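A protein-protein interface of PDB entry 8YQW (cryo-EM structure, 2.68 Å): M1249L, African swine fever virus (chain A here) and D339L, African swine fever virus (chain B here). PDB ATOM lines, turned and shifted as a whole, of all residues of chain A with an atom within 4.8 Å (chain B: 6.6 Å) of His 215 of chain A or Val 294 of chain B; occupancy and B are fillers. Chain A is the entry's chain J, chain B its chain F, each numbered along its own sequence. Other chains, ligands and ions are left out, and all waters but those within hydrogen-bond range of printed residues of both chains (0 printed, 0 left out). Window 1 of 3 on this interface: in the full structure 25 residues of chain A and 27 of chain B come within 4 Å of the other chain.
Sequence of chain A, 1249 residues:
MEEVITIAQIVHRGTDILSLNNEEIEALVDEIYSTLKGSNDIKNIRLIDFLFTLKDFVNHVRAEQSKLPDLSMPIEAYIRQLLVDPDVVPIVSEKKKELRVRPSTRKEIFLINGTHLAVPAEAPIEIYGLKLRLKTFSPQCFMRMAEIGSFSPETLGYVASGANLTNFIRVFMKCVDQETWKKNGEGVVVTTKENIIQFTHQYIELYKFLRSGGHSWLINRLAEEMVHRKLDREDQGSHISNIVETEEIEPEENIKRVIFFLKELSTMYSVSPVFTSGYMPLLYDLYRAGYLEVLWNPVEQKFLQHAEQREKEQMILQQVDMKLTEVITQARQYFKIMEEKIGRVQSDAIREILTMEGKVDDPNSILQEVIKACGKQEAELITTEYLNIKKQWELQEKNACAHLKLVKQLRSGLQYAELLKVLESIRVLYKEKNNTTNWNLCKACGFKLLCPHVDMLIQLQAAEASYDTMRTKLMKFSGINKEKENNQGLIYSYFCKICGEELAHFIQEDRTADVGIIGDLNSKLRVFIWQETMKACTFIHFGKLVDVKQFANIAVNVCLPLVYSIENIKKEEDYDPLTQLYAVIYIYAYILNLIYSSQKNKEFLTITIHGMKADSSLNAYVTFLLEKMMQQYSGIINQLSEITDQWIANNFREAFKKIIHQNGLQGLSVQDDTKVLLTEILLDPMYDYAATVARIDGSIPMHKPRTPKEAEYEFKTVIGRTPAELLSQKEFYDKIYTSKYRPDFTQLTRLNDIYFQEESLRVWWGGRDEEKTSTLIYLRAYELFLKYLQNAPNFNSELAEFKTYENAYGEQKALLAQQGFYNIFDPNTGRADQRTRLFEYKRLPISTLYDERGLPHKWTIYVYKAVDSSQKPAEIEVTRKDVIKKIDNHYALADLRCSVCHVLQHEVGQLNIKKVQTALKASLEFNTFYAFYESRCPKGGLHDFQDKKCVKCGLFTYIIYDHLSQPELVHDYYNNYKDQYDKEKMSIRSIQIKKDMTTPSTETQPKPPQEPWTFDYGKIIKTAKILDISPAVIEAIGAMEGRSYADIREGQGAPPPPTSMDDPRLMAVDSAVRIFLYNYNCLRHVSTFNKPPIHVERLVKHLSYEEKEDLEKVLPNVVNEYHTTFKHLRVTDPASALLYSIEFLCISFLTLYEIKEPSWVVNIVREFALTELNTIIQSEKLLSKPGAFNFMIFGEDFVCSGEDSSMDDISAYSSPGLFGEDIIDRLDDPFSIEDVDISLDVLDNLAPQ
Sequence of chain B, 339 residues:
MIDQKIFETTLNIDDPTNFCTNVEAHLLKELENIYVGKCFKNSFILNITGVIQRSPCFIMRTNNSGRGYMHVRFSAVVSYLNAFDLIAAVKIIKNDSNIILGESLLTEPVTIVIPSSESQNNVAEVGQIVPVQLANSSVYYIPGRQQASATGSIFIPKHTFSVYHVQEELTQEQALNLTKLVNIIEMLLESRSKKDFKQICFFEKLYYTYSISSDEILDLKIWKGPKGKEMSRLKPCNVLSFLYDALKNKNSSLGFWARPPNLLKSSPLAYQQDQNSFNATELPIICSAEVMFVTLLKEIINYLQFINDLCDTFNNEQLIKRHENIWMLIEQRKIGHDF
O of Val 291 of chain B lies within hydrogen-bond range of OG1 of Thr 295 of chain B, at 2.9 Å.
O of Phe 209 of chain A lies within hydrogen-bond range of OG of Ser 212 of chain A, at 2.7 Å.
OG of Ser 212 of chain A lies within hydrogen-bond range of O of Gly 214 of chain A, at 2.9 Å.
His 215 of chain A touches just one residue of chain B: Val 294 (3.8 Å).
Of the printed residues of chain B, Trp 217 of chain A touches Leu 181 (3.6 Å).
Ile 219 of chain A touches none of the printed residues of chain B.
Printed residues of chain A within 4 Å of Glu 290 of chain B: Leu 218 (3.3 Å).
Of the printed residues of chain A, Val 294 of chain B touches Gly 214 (3.5 Å), His 215 (3.8 Å) and Leu 218 (3.9 Å).
The nearest printed residue of chain B that does not touch His 215 of chain A is Lys 298 of chain B (6.6 Å).
The nearest residue of chain A that does not touch Val 294 of chain B is Phe 209 of chain A (4.4 Å).
Hydrophobic or aromatic side chains of chain A that line the printed part of chain B: Phe 168, Phe 209, Trp 217 and Leu 218.
Hydrophobic or aromatic side chains of chain B that line the printed part of chain A: Leu 181, Val 291 and Val 294.
Among the printed residues, 10 pairs touch across the chains.
Among the printed residues, no Asp or Glu carboxylate lies within 4 Å of a Lys or Arg side-chain nitrogen of the other chain.
Among the printed residues, merely in contact across the chains: Leu 218 of chain A with Glu 290 of chain B (3.3 Å), Gly 214 of chain A with Val 294 of chain B (3.5 Å), Trp 217 of chain A with Leu 181 of chain B (3.6 Å), Phe 209 of chain A with Val 291 of chain B (3.6 Å), Phe 168 of chain A with Val 291 of chain B (3.6 Å), His 215 of chain A with Val 294 of chain B (3.8 Å), Gly 214 of chain A with Lys 298 of chain B (3.9 Å), Phe 209 of chain A with Thr 295 of chain B (3.9 Å), Leu 218 of chain A with Val 294 of chain B (3.9 Å) and Gly 213 of chain A with Lys 298 of chain B (3.99 Å).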
ATOM      1  N   PRO A 153     -19.350 -28.062  13.222  1.00  0.00           N
ATOM      2  CA  PRO A 153     -19.690 -28.129  14.652  1.00  0.00           C
ATOM      3  C   PRO A 153     -20.505 -29.355  15.021  1.00  0.00           C
ATOM      4  O   PRO A 153     -20.362 -29.864  16.138  1.00  0.00           O
ATOM      5  CB  PRO A 153     -20.481 -26.835  14.882  1.00  0.00           C
ATOM      6  CG  PRO A 153     -19.983 -25.906  13.839  1.00  0.00           C
ATOM      7  CD  PRO A 153     -19.690 -26.755  12.636  1.00  0.00           C
ATOM      8  N   GLY A 157     -19.295 -31.871  17.917  1.00  0.00           N
ATOM      9  CA  GLY A 157     -20.110 -32.168  19.082  1.00  0.00           C
ATOM     10  C   GLY A 157     -20.468 -33.637  19.194  1.00  0.00           C
ATOM     11  O   GLY A 157     -20.534 -34.184  20.298  1.00  0.00           O
ATOM     12  N   PHE A 168     -24.399 -34.359  25.566  1.00  0.00           N
ATOM     13  CA  PHE A 168     -25.647 -33.939  24.936  1.00  0.00           C
ATOM     14  C   PHE A 168     -26.432 -35.125  24.386  1.00  0.00           C
ATOM     15  O   PHE A 168     -27.663 -35.176  24.518  1.00  0.00           O
ATOM     16  CB  PHE A 168     -25.354 -32.923  23.836  1.00  0.00           C
ATOM     17  CG  PHE A 168     -24.669 -31.684  24.331  1.00  0.00           C
ATOM     18  CD1 PHE A 168     -25.303 -30.839  25.225  1.00  0.00           C
ATOM     19  CD2 PHE A 168     -23.388 -31.370  23.915  1.00  0.00           C
ATOM     20  CE1 PHE A 168     -24.677 -29.702  25.687  1.00  0.00           C
ATOM     21  CE2 PHE A 168     -22.758 -30.234  24.375  1.00  0.00           C
ATOM     22  CZ  PHE A 168     -23.403 -29.399  25.262  1.00  0.00           C
ATOM     23  N   PHE A 209     -30.396 -29.498  17.788  1.00  0.00           N
ATOM     24  CA  PHE A 209     -29.527 -28.797  18.728  1.00  0.00           C
ATOM     25  C   PHE A 209     -28.080 -28.798  18.250  1.00  0.00           C
ATOM     26  O   PHE A 209     -27.377 -27.791  18.389  1.00  0.00           O
ATOM     27  CB  PHE A 209     -29.634 -29.434  20.113  1.00  0.00           C
ATOM     28  CG  PHE A 209     -28.722 -28.822  21.134  1.00  0.00           C
ATOM     29  CD1 PHE A 209     -28.892 -27.509  21.537  1.00  0.00           C
ATOM     30  CD2 PHE A 209     -27.699 -29.563  21.703  1.00  0.00           C
ATOM     31  CE1 PHE A 209     -28.053 -26.944  22.480  1.00  0.00           C
ATOM     32  CE2 PHE A 209     -26.860 -29.006  22.646  1.00  0.00           C
ATOM     33  CZ  PHE A 209     -27.038 -27.694  23.035  1.00  0.00           C
ATOM     34  N   LEU A 210     -27.617 -29.919  17.689  1.00  0.00           N
ATOM     35  CA  LEU A 210     -26.225 -30.001  17.254  1.00  0.00           C
ATOM     36  C   LEU A 210     -25.925 -29.032  16.118  1.00  0.00           C
ATOM     37  O   LEU A 210     -24.799 -28.534  16.012  1.00  0.00           O
ATOM     38  CB  LEU A 210     -25.884 -31.428  16.825  1.00  0.00           C
ATOM     39  CG  LEU A 210     -25.771 -32.479  17.928  1.00  0.00           C
ATOM     40  CD1 LEU A 210     -25.154 -33.750  17.379  1.00  0.00           C
ATOM     41  CD2 LEU A 210     -24.967 -31.952  19.099  1.00  0.00           C
ATOM     42  N   SER A 212     -27.651 -26.135  15.667  1.00  0.00           N
ATOM     43  CA  SER A 212     -28.169 -24.811  15.971  1.00  0.00           C
ATOM     44  C   SER A 212     -27.039 -23.848  16.332  1.00  0.00           C
ATOM     45  O   SER A 212     -25.867 -24.221  16.430  1.00  0.00           O
ATOM     46  CB  SER A 212     -29.183 -24.884  17.113  1.00  0.00           C
ATOM     47  OG  SER A 212     -28.569 -25.324  18.312  1.00  0.00           O
ATOM     48  N   GLY A 213     -27.413 -22.580  16.517  1.00  0.00           N
ATOM     49  CA  GLY A 213     -26.448 -21.591  16.968  1.00  0.00           C
ATOM     50  C   GLY A 213     -25.856 -21.948  18.314  1.00  0.00           C
ATOM     51  O   GLY A 213     -24.651 -21.815  18.537  1.00  0.00           O
ATOM     52  N   GLY A 214     -26.701 -22.405  19.235  1.00  0.00           N
ATOM     53  CA  GLY A 214     -26.196 -23.026  20.439  1.00  0.00           C
ATOM     54  C   GLY A 214     -25.485 -24.327  20.122  1.00  0.00           C
ATOM     55  O   GLY A 214     -25.783 -25.002  19.136  1.00  0.00           O
ATOM     56  N   HIS A 215     -24.506 -24.658  20.965  1.00  0.00           N
ATOM     57  CA  HIS A 215     -23.613 -25.800  20.780  1.00  0.00           C
ATOM     58  C   HIS A 215     -22.660 -25.563  19.612  1.00  0.00           C
ATOM     59  O   HIS A 215     -21.742 -26.354  19.384  1.00  0.00           O
ATOM     60  CB  HIS A 215     -24.406 -27.098  20.583  1.00  0.00           C
ATOM     61  CG  HIS A 215     -23.549 -28.297  20.322  1.00  0.00           C
ATOM     62  ND1 HIS A 215     -22.861 -28.951  21.320  1.00  0.00           N
ATOM     63  CD2 HIS A 215     -23.252 -28.944  19.172  1.00  0.00           C
ATOM     64  CE1 HIS A 215     -22.184 -29.958  20.797  1.00  0.00           C
ATOM     65  NE2 HIS A 215     -22.404 -29.975  19.495  1.00  0.00           N
ATOM     66  N   SER A 216     -22.846 -24.464  18.883  1.00  0.00           N
ATOM     67  CA  SER A 216     -21.841 -24.016  17.930  1.00  0.00           C
ATOM     68  C   SER A 216     -20.841 -23.089  18.611  1.00  0.00           C
ATOM     69  O   SER A 216     -19.631 -23.225  18.418  1.00  0.00           O
ATOM     70  CB  SER A 216     -22.502 -23.315  16.740  1.00  0.00           C
ATOM     71  OG  SER A 216     -23.279 -24.224  15.981  1.00  0.00           O
ATOM     72  N   TRP A 217     -21.343 -22.147  19.412  1.00  0.00           N
ATOM     73  CA  TRP A 217     -20.477 -21.402  20.315  1.00  0.00           C
ATOM     74  C   TRP A 217     -19.805 -22.333  21.313  1.00  0.00           C
ATOM     75  O   TRP A 217     -18.604 -22.212  21.580  1.00  0.00           O
ATOM     76  CB  TRP A 217     -21.289 -20.329  21.045  1.00  0.00           C
ATOM     77  CG  TRP A 217     -20.570 -19.688  22.193  1.00  0.00           C
ATOM     78  CD1 TRP A 217     -19.772 -18.583  22.146  1.00  0.00           C
ATOM     79  CD2 TRP A 217     -20.596 -20.105  23.563  1.00  0.00           C
ATOM     80  NE1 TRP A 217     -19.294 -18.291  23.399  1.00  0.00           N
ATOM     81  CE2 TRP A 217     -19.785 -19.211  24.287  1.00  0.00           C
ATOM     82  CE3 TRP A 217     -21.224 -21.151  24.247  1.00  0.00           C
ATOM     83  CZ2 TRP A 217     -19.585 -19.329  25.659  1.00  0.00           C
ATOM     84  CZ3 TRP A 217     -21.023 -21.268  25.608  1.00  0.00           C
ATOM     85  CH2 TRP A 217     -20.212 -20.362  26.301  1.00  0.00           C
ATOM     86  N   LEU A 218     -20.566 -23.285  21.856  1.00  0.00           N
ATOM     87  CA  LEU A 218     -20.049 -24.158  22.904  1.00  0.00           C
ATOM     88  C   LEU A 218     -18.930 -25.051  22.383  1.00  0.00           C
ATOM     89  O   LEU A 218     -17.851 -25.115  22.980  1.00  0.00           O
ATOM     90  CB  LEU A 218     -21.188 -24.995  23.487  1.00  0.00           C
ATOM     91  CG  LEU A 218     -20.947 -25.755  24.792  1.00  0.00           C
ATOM     92  CD1 LEU A 218     -22.196 -25.723  25.650  1.00  0.00           C
ATOM     93  CD2 LEU A 218     -20.534 -27.190  24.516  1.00  0.00           C
ATOM     94  N   ILE A 219     -19.163 -25.743  21.265  1.00  0.00           N
ATOM     95  CA  ILE A 219     -18.166 -26.691  20.775  1.00  0.00           C
ATOM     96  C   ILE A 219     -16.943 -25.957  20.236  1.00  0.00           C
ATOM     97  O   ILE A 219     -15.809 -26.424  20.396  1.00  0.00           O
ATOM     98  CB  ILE A 219     -18.783 -27.644  19.733  1.00  0.00           C
ATOM     99  CG1 ILE A 219     -17.970 -28.937  19.655  1.00  0.00           C
ATOM    100  CG2 ILE A 219     -18.859 -27.003  18.355  1.00  0.00           C
ATOM    101  CD1 ILE A 219     -17.985 -29.743  20.932  1.00  0.00           C
ATOM    102  N   LEU B 178     -21.272 -20.845  31.147  1.00  0.00           N
ATOM    103  CA  LEU B 178     -22.347 -19.980  30.670  1.00  0.00           C
ATOM    104  C   LEU B 178     -22.164 -18.526  31.080  1.00  0.00           C
ATOM    105  O   LEU B 178     -22.764 -17.639  30.460  1.00  0.00           O
ATOM    106  CB  LEU B 178     -23.693 -20.489  31.182  1.00  0.00           C
ATOM    107  CG  LEU B 178     -24.123 -21.864  30.672  1.00  0.00           C
ATOM    108  CD1 LEU B 178     -25.496 -22.215  31.200  1.00  0.00           C
ATOM    109  CD2 LEU B 178     -24.099 -21.905  29.158  1.00  0.00           C
ATOM    110  N   LEU B 181     -21.376 -16.274  28.099  1.00  0.00           N
ATOM    111  CA  LEU B 181     -22.536 -15.769  27.371  1.00  0.00           C
ATOM    112  C   LEU B 181     -23.275 -14.722  28.190  1.00  0.00           C
ATOM    113  O   LEU B 181     -23.835 -13.768  27.638  1.00  0.00           O
ATOM    114  CB  LEU B 181     -23.469 -16.921  27.000  1.00  0.00           C
ATOM    115  CG  LEU B 181     -22.958 -17.871  25.919  1.00  0.00           C
ATOM    116  CD1 LEU B 181     -23.847 -19.096  25.821  1.00  0.00           C
ATOM    117  CD2 LEU B 181     -22.885 -17.149  24.583  1.00  0.00           C
ATOM    118  N   ALA B 289     -30.350 -28.796  31.791  1.00  0.00           N
ATOM    119  CA  ALA B 289     -30.381 -27.357  32.025  1.00  0.00           C
ATOM    120  C   ALA B 289     -29.398 -26.628  31.121  1.00  0.00           C
ATOM    121  O   ALA B 289     -29.667 -25.504  30.680  1.00  0.00           O
ATOM    122  CB  ALA B 289     -30.084 -27.055  33.493  1.00  0.00           C
ATOM    123  N   GLU B 290     -28.251 -27.249  30.840  1.00  0.00           N
ATOM    124  CA  GLU B 290     -27.251 -26.605  29.996  1.00  0.00           C
ATOM    125  C   GLU B 290     -27.779 -26.374  28.585  1.00  0.00           C
ATOM    126  O   GLU B 290     -27.562 -25.304  28.008  1.00  0.00           O
ATOM    127  CB  GLU B 290     -25.976 -27.445  29.960  1.00  0.00           C
ATOM    128  CG  GLU B 290     -24.825 -26.780  29.232  1.00  0.00           C
ATOM    129  CD  GLU B 290     -23.626 -27.692  29.091  1.00  0.00           C
ATOM    130  OE1 GLU B 290     -23.723 -28.866  29.506  1.00  0.00           O
ATOM    131  OE2 GLU B 290     -22.592 -27.240  28.559  1.00  0.00           O
ATOM    132  N   VAL B 291     -28.483 -27.357  28.022  1.00  0.00           N
ATOM    133  CA  VAL B 291     -29.000 -27.225  26.660  1.00  0.00           C
ATOM    134  C   VAL B 291     -29.975 -26.059  26.566  1.00  0.00           C
ATOM    135  O   VAL B 291     -29.863 -25.198  25.684  1.00  0.00           O
ATOM    136  CB  VAL B 291     -29.660 -28.541  26.210  1.00  0.00           C
ATOM    137  CG1 VAL B 291     -30.362 -28.351  24.877  1.00  0.00           C
ATOM    138  CG2 VAL B 291     -28.628 -29.649  26.117  1.00  0.00           C
ATOM    139  N   MET B 292     -30.949 -26.015  27.478  1.00  0.00           N
ATOM    140  CA  MET B 292     -31.970 -24.974  27.432  1.00  0.00           C
ATOM    141  C   MET B 292     -31.378 -23.602  27.731  1.00  0.00           C
ATOM    142  O   MET B 292     -31.749 -22.609  27.096  1.00  0.00           O
ATOM    143  CB  MET B 292     -33.097 -25.314  28.408  1.00  0.00           C
ATOM    144  CG  MET B 292     -34.158 -24.236  28.582  1.00  0.00           C
ATOM    145  SD  MET B 292     -33.749 -23.080  29.898  1.00  0.00           S
ATOM    146  CE  MET B 292     -33.523 -24.234  31.240  1.00  0.00           C
ATOM    147  N   PHE B 293     -30.470 -23.524  28.710  1.00  0.00           N
ATOM    148  CA  PHE B 293     -29.787 -22.262  28.976  1.00  0.00           C
ATOM    149  C   PHE B 293     -29.021 -21.777  27.756  1.00  0.00           C
ATOM    150  O   PHE B 293     -29.101 -20.596  27.401  1.00  0.00           O
ATOM    151  CB  PHE B 293     -28.848 -22.399  30.173  1.00  0.00           C
ATOM    152  CG  PHE B 293     -29.549 -22.472  31.500  1.00  0.00           C
ATOM    153  CD1 PHE B 293     -30.863 -22.062  31.630  1.00  0.00           C
ATOM    154  CD2 PHE B 293     -28.888 -22.947  32.619  1.00  0.00           C
ATOM    155  CE1 PHE B 293     -31.503 -22.116  32.856  1.00  0.00           C
ATOM    156  CE2 PHE B 293     -29.529 -23.013  33.843  1.00  0.00           C
ATOM    157  CZ  PHE B 293     -30.837 -22.598  33.959  1.00  0.00           C
ATOM    158  N   VAL B 294     -28.285 -22.668  27.092  1.00  0.00           N
ATOM    159  CA  VAL B 294     -27.530 -22.268  25.908  1.00  0.00           C
ATOM    160  C   VAL B 294     -28.475 -21.772  24.824  1.00  0.00           C
ATOM    161  O   VAL B 294     -28.238 -20.731  24.200  1.00  0.00           O
ATOM    162  CB  VAL B 294     -26.661 -23.438  25.409  1.00  0.00           C
ATOM    163  CG1 VAL B 294     -26.245 -23.209  23.976  1.00  0.00           C
ATOM    164  CG2 VAL B 294     -25.443 -23.604  26.290  1.00  0.00           C
ATOM    165  N   THR B 295     -29.570 -22.501  24.594  1.00  0.00           N
ATOM    166  CA  THR B 295     -30.501 -22.119  23.538  1.00  0.00           C
ATOM    167  C   THR B 295     -31.119 -20.753  23.813  1.00  0.00           C
ATOM    168  O   THR B 295     -31.085 -19.859  22.958  1.00  0.00           O
ATOM    169  CB  THR B 295     -31.592 -23.177  23.391  1.00  0.00           C
ATOM    170  OG1 THR B 295     -30.992 -24.459  23.173  1.00  0.00           O
ATOM    171  CG2 THR B 295     -32.489 -22.841  22.217  1.00  0.00           C
ATOM    172  N   LEU B 296     -31.685 -20.570  25.010  1.00  0.00           N
ATOM    173  CA  LEU B 296     -32.336 -19.304  25.331  1.00  0.00           C
ATOM    174  C   LEU B 296     -31.339 -18.154  25.347  1.00  0.00           C
ATOM    175  O   LEU B 296     -31.632 -17.065  24.837  1.00  0.00           O
ATOM    176  CB  LEU B 296     -33.057 -19.406  26.676  1.00  0.00           C
ATOM    177  CG  LEU B 296     -34.161 -20.457  26.788  1.00  0.00           C
ATOM    178  CD1 LEU B 296     -34.999 -20.212  28.031  1.00  0.00           C
ATOM    179  CD2 LEU B 296     -35.033 -20.460  25.543  1.00  0.00           C
ATOM    180  N   LEU B 297     -30.150 -18.375  25.916  1.00  0.00           N
ATOM    181  CA  LEU B 297     -29.129 -17.338  25.906  1.00  0.00           C
ATOM    182  C   LEU B 297     -28.790 -16.933  24.481  1.00  0.00           C
ATOM    183  O   LEU B 297     -28.997 -15.778  24.097  1.00  0.00           O
ATOM    184  CB  LEU B 297     -27.884 -17.822  26.652  1.00  0.00           C
ATOM    185  CG  LEU B 297     -27.937 -17.695  28.177  1.00  0.00           C
ATOM    186  CD1 LEU B 297     -26.650 -18.199  28.814  1.00  0.00           C
ATOM    187  CD2 LEU B 297     -28.212 -16.256  28.581  1.00  0.00           C
ATOM    188  N   LYS B 298     -28.344 -17.890  23.658  1.00  0.00           N
ATOM    189  CA  LYS B 298     -27.978 -17.578  22.281  1.00  0.00           C
ATOM    190  C   LYS B 298     -29.116 -16.890  21.540  1.00  0.00           C
ATOM    191  O   LYS B 298     -28.867 -16.009  20.711  1.00  0.00           O
ATOM    192  CB  LYS B 298     -27.553 -18.851  21.549  1.00  0.00           C
ATOM    193  CG  LYS B 298     -27.294 -18.660  20.064  1.00  0.00           C
ATOM    194  CD  LYS B 298     -26.158 -17.681  19.821  1.00  0.00           C
ATOM    195  CE  LYS B 298     -25.974 -17.412  18.336  1.00  0.00           C
ATOM    196  NZ  LYS B 298     -25.023 -16.297  18.082  1.00  0.00           N
ATOM    197  N   GLU B 299     -30.366 -17.241  21.852  1.00  0.00           N
ATOM    198  CA  GLU B 299     -31.492 -16.498  21.298  1.00  0.00           C
ATOM    199  C   GLU B 299     -31.463 -15.041  21.745  1.00  0.00           C
ATOM    200  O   GLU B 299     -31.719 -14.131  20.944  1.00  0.00           O
ATOM    201  CB  GLU B 299     -32.803 -17.163  21.712  1.00  0.00           C
ATOM    202  CG  GLU B 299     -34.039 -16.538  21.101  1.00  0.00           C
ATOM    203  CD  GLU B 299     -35.313 -17.240  21.522  1.00  0.00           C
ATOM    204  OE1 GLU B 299     -35.227 -18.202  22.313  1.00  0.00           O
ATOM    205  OE2 GLU B 299     -36.400 -16.832  21.063  1.00  0.00           O
ATOM    206  N   ILE B 301     -28.801 -13.250  22.756  1.00  0.00           N
ATOM    207  CA  ILE B 301     -27.713 -12.606  22.010  1.00  0.00           C
ATOM    208  C   ILE B 301     -28.156 -12.283  20.588  1.00  0.00           C
ATOM    209  O   ILE B 301     -27.911 -11.183  20.081  1.00  0.00           O
ATOM    210  CB  ILE B 301     -26.417 -13.447  22.003  1.00  0.00           C
ATOM    211  CG1 ILE B 301     -25.793 -13.643  23.391  1.00  0.00           C
ATOM    212  CG2 ILE B 301     -25.389 -12.832  21.066  1.00  0.00           C
ATOM    213  CD1 ILE B 301     -26.244 -14.820  24.165  1.00  0.00           C
